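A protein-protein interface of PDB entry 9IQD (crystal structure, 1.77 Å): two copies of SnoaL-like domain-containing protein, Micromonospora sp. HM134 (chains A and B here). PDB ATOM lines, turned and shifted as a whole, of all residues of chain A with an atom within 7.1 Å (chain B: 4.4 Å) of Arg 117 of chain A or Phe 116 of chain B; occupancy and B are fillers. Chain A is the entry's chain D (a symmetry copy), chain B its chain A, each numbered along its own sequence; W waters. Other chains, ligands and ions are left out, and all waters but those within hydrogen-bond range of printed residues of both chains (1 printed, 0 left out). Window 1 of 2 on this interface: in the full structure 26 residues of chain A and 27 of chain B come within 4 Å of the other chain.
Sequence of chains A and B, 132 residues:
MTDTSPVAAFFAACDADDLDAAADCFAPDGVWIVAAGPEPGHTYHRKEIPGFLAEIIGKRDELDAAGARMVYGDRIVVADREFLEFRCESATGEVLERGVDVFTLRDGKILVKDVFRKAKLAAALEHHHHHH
The side-chain carboxylate of Asp 114 of chain B lies within salt-bridge range of the guanidinium group of Arg 98 of chain A (2.8 Å).
N of Arg 117 of chain B is in hydrogen-bond range of O of Arg 117 of chain A (3.0 Å).
The backbone carbonyl oxygen of Val 115 of chain B sits at hydrogen-bond distance from the side-chain amino group of Lys 118 of chain A.
The backbone carbonyl oxygen of Ala 35 of chain B lies within hydrogen-bond range of the backbone NH of Ala 119 of chain A, at 2.9 Å.
The side-chain amino group (NZ) of Lys 118 of chain A is in salt-bridge range of the side-chain carboxylate (OD1) of Asp 114 of chain B (2.8 Å).
Of the printed residues of chain B, Gly 99 of chain A touches Phe 116.
Of the printed residues of chain B, Phe 116 of chain A touches Gly 99 (3.6 Å), Val 100 (3.7 Å), Phe 116 (3.5 Å) and Arg 117 (3.7 Å).
Arg 117 of chain A touches just these residues of chain B: Phe 116 (3.7 Å) and Arg 117 (3.0 Å).
Of the printed residues of chain A, Gly 99 of chain B touches Phe 116.
Of the printed residues of chain A, Val 102 of chain B touches Glu 85 (3.8 Å).
Of chain A, only Glu 85, Arg 98, Gly 99, Val 100, Phe 116, Arg 117 and Lys 118 come within 4 Å of Phe 116 of chain B.
The nearest residue of chain B that does not touch Arg 117 of chain A is Ala 35 of chain B (4.2 Å).
Water W1 bridges OD2 of Asp 114 of chain B (2.7 Å) and OE2 of Glu 85 of chain A (3.0 Å).
Among the printed residues, pairs that only touch across the chains: Glu 85 of chain A with Val 102 of chain B, Glu 85 of chain A with Phe 116 of chain B, Arg 98 of chain A with Phe 116 of chain B, Gly 99 of chain A with Phe 116 of chain B, Val 100 of chain A with Val 100 of chain B, Val 100 of chain A with Phe 116 of chain B, Phe 116 of chain A with Gly 99 of chain B, Phe 116 of chain A with Val 100 of chain B, Phe 116 of chain A with Phe 116 of chain B, Phe 116 of chain A with Arg 117 of chain B, Arg 117 of chain A with Phe 116 of chain B, Lys 118 of chain A with Ala 35 of chain B and Lys 118 of chain A with Phe 116 of chain B.
Val 100 of chain B touches its own counterpart, Val 100 of chain A.
Phe 116 of chain B touches its own counterpart, Phe 116 of chain A.
Phe 116 of chain A touches Arg 117 of chain B, and with the chains exchanged Arg 117 of chain A touches Phe 116 of chain B.
Arg 117 of chain A touches its own counterpart, Arg 117 of chain B.
6 positions are printed for both chains.
Hydrophobic or aromatic side chains of chain A that line the printed part of chain B: Val 100 and Phe 116.
Hydrophobic or aromatic side chains of chain B within 4 Å of the printed part of chain A: Val 100, Val 102 and Phe 116.
Along chain B the printed residues that touch a printed residue of chain A span positions 35 to 117.
Among the printed residues, Asp or Glu carboxylates within 4 Å of a Lys or Arg side-chain nitrogen of the other chain: Arg 98 of chain A with Asp 114 of chain B (2.8 Å) and Lys 118 of chain A with Asp 114 of chain B (2.8 Å).
The backbone NH of Val 100 of chain B lies within hydrogen-bond range of the backbone carbonyl oxygen of Phe 116 of chain B (2.9 Å).
The backbone carbonyl oxygen (O) of Phe 86 of chain A sits at hydrogen-bond distance from the backbone NH (N) of Gly 99 of chain A (3.0 Å).
N of Lys 118 of chain A sits at hydrogen-bond distance from O of Arg 98 of chain A (2.9 Å).
OE1 of Glu 97 of chain A lies within salt-bridge range of NH1 of Arg 117 of chain A.
OE1 of Glu 85 of chain A is in salt-bridge range of NH1 of Arg 98 of chain A (3.9 Å).
The backbone NH (N) of Val 100 of chain A lies within hydrogen-bond range of the backbone carbonyl oxygen (O) of Phe 116 of chain A, at 2.8 Å.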
ATOM      1  N   VAL A  34       7.061  31.602  19.085  1.00  0.00           N
ATOM      2  CA  VAL A  34       5.895  32.175  19.721  1.00  0.00           C
ATOM      3  C   VAL A  34       4.947  32.748  18.665  1.00  0.00           C
ATOM      4  O   VAL A  34       5.287  32.926  17.488  1.00  0.00           O
ATOM      5  CB  VAL A  34       6.268  33.238  20.769  1.00  0.00           C
ATOM      6  CG1 VAL A  34       7.051  32.576  21.927  1.00  0.00           C
ATOM      7  CG2 VAL A  34       7.041  34.409  20.137  1.00  0.00           C
ATOM      8  N   ALA A  35       3.722  33.016  19.101  1.00  0.00           N
ATOM      9  CA  ALA A  35       2.672  33.364  18.149  1.00  0.00           C
ATOM     10  C   ALA A  35       2.911  34.723  17.504  1.00  0.00           C
ATOM     11  O   ALA A  35       2.593  34.901  16.329  1.00  0.00           O
ATOM     12  CB  ALA A  35       1.305  33.348  18.839  1.00  0.00           C
ATOM     13  N   ALA A  36       3.433  35.701  18.253  1.00  0.00           N
ATOM     14  CA  ALA A  36       3.510  37.088  17.790  1.00  0.00           C
ATOM     15  C   ALA A  36       4.952  37.504  17.520  1.00  0.00           C
ATOM     16  O   ALA A  36       5.861  37.165  18.279  1.00  0.00           O
ATOM     17  CB  ALA A  36       2.902  38.053  18.815  1.00  0.00           C
ATOM     18  N   LYS A  59       5.205  34.959  34.414  1.00  0.00           N
ATOM     19  CA  LYS A  59       3.847  35.322  34.025  1.00  0.00           C
ATOM     20  C   LYS A  59       2.846  34.282  34.502  1.00  0.00           C
ATOM     21  O   LYS A  59       1.775  34.633  35.015  1.00  0.00           O
ATOM     22  CB  LYS A  59       3.751  35.495  32.509  1.00  0.00           C
ATOM     23  CG  LYS A  59       2.301  35.495  32.013  1.00  0.00           C
ATOM     24  CD  LYS A  59       2.177  35.724  30.514  1.00  0.00           C
ATOM     25  CE  LYS A  59       0.758  35.406  30.048  1.00  0.00           C
ATOM     26  NZ  LYS A  59       0.528  35.775  28.624  1.00  0.00           N
ATOM     27  N   GLU A  85      -4.103  21.778  22.469  1.00  0.00           N
ATOM     28  CA  GLU A  85      -4.845  23.011  22.716  1.00  0.00           C
ATOM     29  C   GLU A  85      -4.693  23.456  24.169  1.00  0.00           C
ATOM     30  O   GLU A  85      -4.499  22.640  25.084  1.00  0.00           O
ATOM     31  CB  GLU A  85      -6.324  22.830  22.377  1.00  0.00           C
ATOM     32  CG  GLU A  85      -6.572  22.750  20.885  1.00  0.00           C
ATOM     33  CD  GLU A  85      -8.049  22.853  20.524  1.00  0.00           C
ATOM     34  OE1 GLU A  85      -8.720  23.853  20.876  1.00  0.00           O
ATOM     35  OE2 GLU A  85      -8.547  21.909  19.885  1.00  0.00           O
ATOM     36  N   PHE A  86      -4.757  24.768  24.372  1.00  0.00           N
ATOM     37  CA  PHE A  86      -4.602  25.336  25.700  1.00  0.00           C
ATOM     38  C   PHE A  86      -5.485  26.567  25.811  1.00  0.00           C
ATOM     39  O   PHE A  86      -5.760  27.250  24.819  1.00  0.00           O
ATOM     40  CB  PHE A  86      -3.142  25.713  26.010  1.00  0.00           C
ATOM     41  CG  PHE A  86      -2.591  26.806  25.117  1.00  0.00           C
ATOM     42  CD1 PHE A  86      -2.796  28.147  25.432  1.00  0.00           C
ATOM     43  CD2 PHE A  86      -1.869  26.481  23.962  1.00  0.00           C
ATOM     44  CE1 PHE A  86      -2.297  29.165  24.617  1.00  0.00           C
ATOM     45  CE2 PHE A  86      -1.367  27.491  23.133  1.00  0.00           C
ATOM     46  CZ  PHE A  86      -1.588  28.835  23.464  1.00  0.00           C
ATOM     47  N   CYS A  88      -6.262  29.808  28.945  1.00  0.00           N
ATOM     48  CA  CYS A  88      -6.119  30.378  30.271  1.00  0.00           C
ATOM     49  C   CYS A  88      -7.446  31.028  30.635  1.00  0.00           C
ATOM     50  O   CYS A  88      -7.966  31.843  29.866  1.00  0.00           O
ATOM     51  CB  CYS A  88      -4.986  31.402  30.297  1.00  0.00           C
ATOM     52  SG  CYS A  88      -4.682  32.047  31.958  1.00  0.00           S
ATOM     53  N   LEU A  96      -9.038  34.198  28.982  1.00  0.00           N
ATOM     54  CA  LEU A  96      -7.992  35.211  28.908  1.00  0.00           C
ATOM     55  C   LEU A  96      -7.099  35.008  27.694  1.00  0.00           C
ATOM     56  O   LEU A  96      -6.673  35.981  27.067  1.00  0.00           O
ATOM     57  CB  LEU A  96      -7.131  35.165  30.180  1.00  0.00           C
ATOM     58  CG  LEU A  96      -7.932  35.271  31.481  1.00  0.00           C
ATOM     59  CD1 LEU A  96      -7.053  35.005  32.687  1.00  0.00           C
ATOM     60  CD2 LEU A  96      -8.545  36.664  31.532  1.00  0.00           C
ATOM     61  N   GLU A  97      -6.816  33.746  27.366  1.00  0.00           N
ATOM     62  CA  GLU A  97      -5.934  33.345  26.271  1.00  0.00           C
ATOM     63  C   GLU A  97      -6.432  32.024  25.708  1.00  0.00           C
ATOM     64  O   GLU A  97      -6.919  31.170  26.449  1.00  0.00           O
ATOM     65  CB  GLU A  97      -4.480  33.110  26.714  1.00  0.00           C
ATOM     66  CG  GLU A  97      -3.809  34.203  27.501  1.00  0.00           C
ATOM     67  CD  GLU A  97      -2.457  33.752  28.047  1.00  0.00           C
ATOM     68  OE1 GLU A  97      -1.820  32.857  27.437  1.00  0.00           O
ATOM     69  OE2 GLU A  97      -2.037  34.277  29.099  1.00  0.00           O
ATOM     70  N   ARG A  98      -6.262  31.827  24.405  1.00  0.00           N
ATOM     71  CA  ARG A  98      -6.572  30.507  23.866  1.00  0.00           C
ATOM     72  C   ARG A  98      -5.718  30.258  22.634  1.00  0.00           C
ATOM     73  O   ARG A  98      -5.486  31.170  21.840  1.00  0.00           O
ATOM     74  CB  ARG A  98      -8.064  30.370  23.534  1.00  0.00           C
ATOM     75  CG  ARG A  98      -8.464  28.928  23.198  1.00  0.00           C
ATOM     76  CD  ARG A  98      -9.959  28.706  23.334  1.00  0.00           C
ATOM     77  NE  ARG A  98     -10.734  29.214  22.201  1.00  0.00           N
ATOM     78  CZ  ARG A  98     -10.881  28.558  21.059  1.00  0.00           C
ATOM     79  NH1 ARG A  98     -10.221  27.434  20.823  1.00  0.00           N
ATOM     80  NH2 ARG A  98     -11.699  29.046  20.124  1.00  0.00           N
ATOM     81  N   GLY A  99      -5.249  29.025  22.482  1.00  0.00           N
ATOM     82  CA  GLY A  99      -4.425  28.742  21.326  1.00  0.00           C
ATOM     83  C   GLY A  99      -4.187  27.258  21.178  1.00  0.00           C
ATOM     84  O   GLY A  99      -4.879  26.438  21.778  1.00  0.00           O
ATOM     85  N   VAL A 100      -3.203  26.927  20.343  1.00  0.00           N
ATOM     86  CA  VAL A 100      -2.813  25.531  20.145  1.00  0.00           C
ATOM     87  C   VAL A 100      -1.310  25.490  19.914  1.00  0.00           C
ATOM     88  O   VAL A 100      -0.750  26.357  19.243  1.00  0.00           O
ATOM     89  CB  VAL A 100      -3.565  24.872  18.971  1.00  0.00           C
ATOM     90  CG1 VAL A 100      -3.252  25.590  17.640  1.00  0.00           C
ATOM     91  CG2 VAL A 100      -3.190  23.387  18.855  1.00  0.00           C
ATOM     92  N   ASP A 101      -0.654  24.499  20.507  1.00  0.00           N
ATOM     93  CA  ASP A 101       0.763  24.241  20.274  1.00  0.00           C
ATOM     94  C   ASP A 101       0.891  23.124  19.249  1.00  0.00           C
ATOM     95  O   ASP A 101       0.235  22.086  19.383  1.00  0.00           O
ATOM     96  CB  ASP A 101       1.491  23.800  21.552  1.00  0.00           C
ATOM     97  CG  ASP A 101       1.585  24.880  22.610  1.00  0.00           C
ATOM     98  OD1 ASP A 101       1.567  26.079  22.261  1.00  0.00           O
ATOM     99  OD2 ASP A 101       1.710  24.509  23.805  1.00  0.00           O
ATOM    100  N   VAL A 115       3.600  27.954  18.179  1.00  0.00           N
ATOM    101  CA  VAL A 115       2.445  28.384  18.967  1.00  0.00           C
ATOM    102  C   VAL A 115       1.533  29.235  18.089  1.00  0.00           C
ATOM    103  O   VAL A 115       1.993  30.169  17.426  1.00  0.00           O
ATOM    104  CB  VAL A 115       2.873  29.166  20.219  1.00  0.00           C
ATOM    105  CG1 VAL A 115       1.641  29.455  21.074  1.00  0.00           C
ATOM    106  CG2 VAL A 115       3.907  28.361  21.030  1.00  0.00           C
ATOM    107  N   PHE A 116       0.247  28.892  18.063  1.00  0.00           N
ATOM    108  CA  PHE A 116      -0.763  29.644  17.324  1.00  0.00           C
ATOM    109  C   PHE A 116      -1.860  30.066  18.288  1.00  0.00           C
ATOM    110  O   PHE A 116      -2.178  29.338  19.226  1.00  0.00           O
ATOM    111  CB  PHE A 116      -1.398  28.818  16.200  1.00  0.00           C
ATOM    112  CG  PHE A 116      -0.417  28.245  15.227  1.00  0.00           C
ATOM    113  CD1 PHE A 116       0.269  27.074  15.520  1.00  0.00           C
ATOM    114  CD2 PHE A 116      -0.225  28.838  13.997  1.00  0.00           C
ATOM    115  CE1 PHE A 116       1.160  26.538  14.623  1.00  0.00           C
ATOM    116  CE2 PHE A 116       0.651  28.292  13.076  1.00  0.00           C
ATOM    117  CZ  PHE A 116       1.345  27.142  13.385  1.00  0.00           C
ATOM    118  N   ARG A 117      -2.465  31.231  18.055  1.00  0.00           N
ATOM    119  CA  ARG A 117      -3.380  31.771  19.057  1.00  0.00           C
ATOM    120  C   ARG A 117      -4.634  32.380  18.434  1.00  0.00           C
ATOM    121  O   ARG A 117      -4.674  32.718  17.242  1.00  0.00           O
ATOM    122  CB  ARG A 117      -2.689  32.856  19.913  1.00  0.00           C
ATOM    123  CG  ARG A 117      -1.757  32.316  20.970  1.00  0.00           C
ATOM    124  CD  ARG A 117      -1.044  33.418  21.744  1.00  0.00           C
ATOM    125  NE  ARG A 117      -0.050  32.850  22.655  1.00  0.00           N
ATOM    126  CZ  ARG A 117      -0.269  32.587  23.937  1.00  0.00           C
ATOM    127  NH1 ARG A 117      -1.421  32.892  24.518  1.00  0.00           N
ATOM    128  NH2 ARG A 117       0.683  31.988  24.648  1.00  0.00           N
ATOM    129  N   LYS A 118      -5.679  32.474  19.267  1.00  0.00           N
ATOM    130  CA  LYS A 118      -6.750  33.441  19.050  1.00  0.00           C
ATOM    131  C   LYS A 118      -6.280  34.798  19.564  1.00  0.00           C
ATOM    132  O   LYS A 118      -5.413  34.885  20.434  1.00  0.00           O
ATOM    133  CB  LYS A 118      -8.030  33.041  19.789  1.00  0.00           C
ATOM    134  CG  LYS A 118      -8.339  31.555  19.762  1.00  0.00           C
ATOM    135  CD  LYS A 118      -8.618  31.053  18.333  1.00  0.00           C
ATOM    136  CE  LYS A 118     -10.028  31.286  17.891  1.00  0.00           C
ATOM    137  NZ  LYS A 118     -10.407  30.517  16.641  1.00  0.00           N
ATOM    138  N   ALA A 119      -6.861  35.866  19.031  1.00  0.00           N
ATOM    139  CA  ALA A 119      -6.453  37.189  19.479  1.00  0.00           C
ATOM    140  C   ALA A 119      -7.664  38.097  19.529  1.00  0.00           C
ATOM    141  O   ALA A 119      -8.575  37.968  18.720  1.00  0.00           O
ATOM    142  CB  ALA A 119      -5.389  37.805  18.558  1.00  0.00           C
ATOM    143  N   ALA B  35      -9.857  33.535  13.929  1.00  0.00           N
ATOM    144  CA  ALA B  35      -8.800  33.696  14.911  1.00  0.00           C
ATOM    145  C   ALA B  35      -8.979  34.959  15.737  1.00  0.00           C
ATOM    146  O   ALA B  35      -8.617  34.969  16.915  1.00  0.00           O
ATOM    147  CB  ALA B  35      -7.434  33.709  14.222  1.00  0.00           C
ATOM    148  N   GLY B  99      -1.100  30.021   9.840  1.00  0.00           N
ATOM    149  CA  GLY B  99      -1.957  29.566  10.912  1.00  0.00           C
ATOM    150  C   GLY B  99      -2.157  28.073  10.852  1.00  0.00           C
ATOM    151  O   GLY B  99      -1.453  27.356  10.141  1.00  0.00           O
ATOM    152  N   VAL B 100      -3.110  27.602  11.645  1.00  0.00           N
ATOM    153  CA  VAL B 100      -3.484  26.195  11.601  1.00  0.00           C
ATOM    154  C   VAL B 100      -4.981  26.111  11.846  1.00  0.00           C
ATOM    155  O   VAL B 100      -5.525  26.851  12.672  1.00  0.00           O
ATOM    156  CB  VAL B 100      -2.683  25.356  12.625  1.00  0.00           C
ATOM    157  CG1 VAL B 100      -2.979  25.808  14.069  1.00  0.00           C
ATOM    158  CG2 VAL B 100      -3.005  23.873  12.469  1.00  0.00           C
ATOM    159  N   VAL B 102      -8.017  23.673  13.148  1.00  0.00           N
ATOM    160  CA  VAL B 102      -8.307  22.469  13.912  1.00  0.00           C
ATOM    161  C   VAL B 102      -9.779  22.176  13.697  1.00  0.00           C
ATOM    162  O   VAL B 102     -10.636  22.991  14.057  1.00  0.00           O
ATOM    163  CB  VAL B 102      -7.996  22.628  15.407  1.00  0.00           C
ATOM    164  CG1 VAL B 102      -8.324  21.316  16.145  1.00  0.00           C
ATOM    165  CG2 VAL B 102      -6.518  23.031  15.602  1.00  0.00           C
ATOM    166  N   ASP B 114     -11.879  25.609  13.847  1.00  0.00           N
ATOM    167  CA  ASP B 114     -11.280  26.510  14.838  1.00  0.00           C
ATOM    168  C   ASP B 114      -9.951  26.999  14.262  1.00  0.00           C
ATOM    169  O   ASP B 114      -9.012  26.207  14.108  1.00  0.00           O
ATOM    170  CB  ASP B 114     -11.101  25.757  16.165  1.00  0.00           C
ATOM    171  CG  ASP B 114     -11.159  26.666  17.413  1.00  0.00           C
ATOM    172  OD1 ASP B 114     -11.228  27.915  17.291  1.00  0.00           O
ATOM    173  OD2 ASP B 114     -11.167  26.108  18.532  1.00  0.00           O
ATOM    174  N   VAL B 115      -9.857  28.298  13.948  1.00  0.00           N
ATOM    175  CA  VAL B 115      -8.681  28.841  13.261  1.00  0.00           C
ATOM    176  C   VAL B 115      -7.767  29.539  14.265  1.00  0.00           C
ATOM    177  O   VAL B 115      -8.220  30.381  15.047  1.00  0.00           O
ATOM    178  CB  VAL B 115      -9.090  29.826  12.156  1.00  0.00           C
ATOM    179  CG1 VAL B 115      -7.863  30.239  11.384  1.00  0.00           C
ATOM    180  CG2 VAL B 115     -10.145  29.202  11.244  1.00  0.00           C
ATOM    181  N   PHE B 116      -6.472  29.207  14.222  1.00  0.00           N
ATOM    182  CA  PHE B 116      -5.479  29.851  15.068  1.00  0.00           C
ATOM    183  C   PHE B 116      -4.376  30.433  14.198  1.00  0.00           C
ATOM    184  O   PHE B 116      -4.026  29.858  13.165  1.00  0.00           O
ATOM    185  CB  PHE B 116      -4.857  28.853  16.076  1.00  0.00           C
ATOM    186  CG  PHE B 116      -5.860  28.121  16.917  1.00  0.00           C
ATOM    187  CD1 PHE B 116      -6.479  26.966  16.443  1.00  0.00           C
ATOM    188  CD2 PHE B 116      -6.152  28.557  18.203  1.00  0.00           C
ATOM    189  CE1 PHE B 116      -7.411  26.278  17.222  1.00  0.00           C
ATOM    190  CE2 PHE B 116      -7.072  27.860  18.999  1.00  0.00           C
ATOM    191  CZ  PHE B 116      -7.697  26.716  18.502  1.00  0.00           C
ATOM    192  N   ARG B 117      -3.780  31.547  14.625  1.00  0.00           N
ATOM    193  CA  ARG B 117      -2.851  32.224  13.729  1.00  0.00           C
ATOM    194  C   ARG B 117      -1.596  32.717  14.442  1.00  0.00           C
ATOM    195  O   ARG B 117      -1.573  32.903  15.658  1.00  0.00           O
ATOM    196  CB  ARG B 117      -3.534  33.427  13.052  1.00  0.00           C
ATOM    197  CG  ARG B 117      -4.570  33.011  12.010  1.00  0.00           C
ATOM    198  CD  ARG B 117      -5.271  34.211  11.360  1.00  0.00           C
ATOM    199  NE  ARG B 117      -6.336  33.762  10.468  1.00  0.00           N
ATOM    200  CZ  ARG B 117      -6.238  33.697   9.146  1.00  0.00           C
ATOM    201  NH1 ARG B 117      -5.155  34.130   8.503  1.00  0.00           N
ATOM    202  NH2 ARG B 117      -7.249  33.182   8.445  1.00  0.00           N
HETATM  203  O   HOH W   1     -10.673  23.466  18.473  1.00  0.00           O
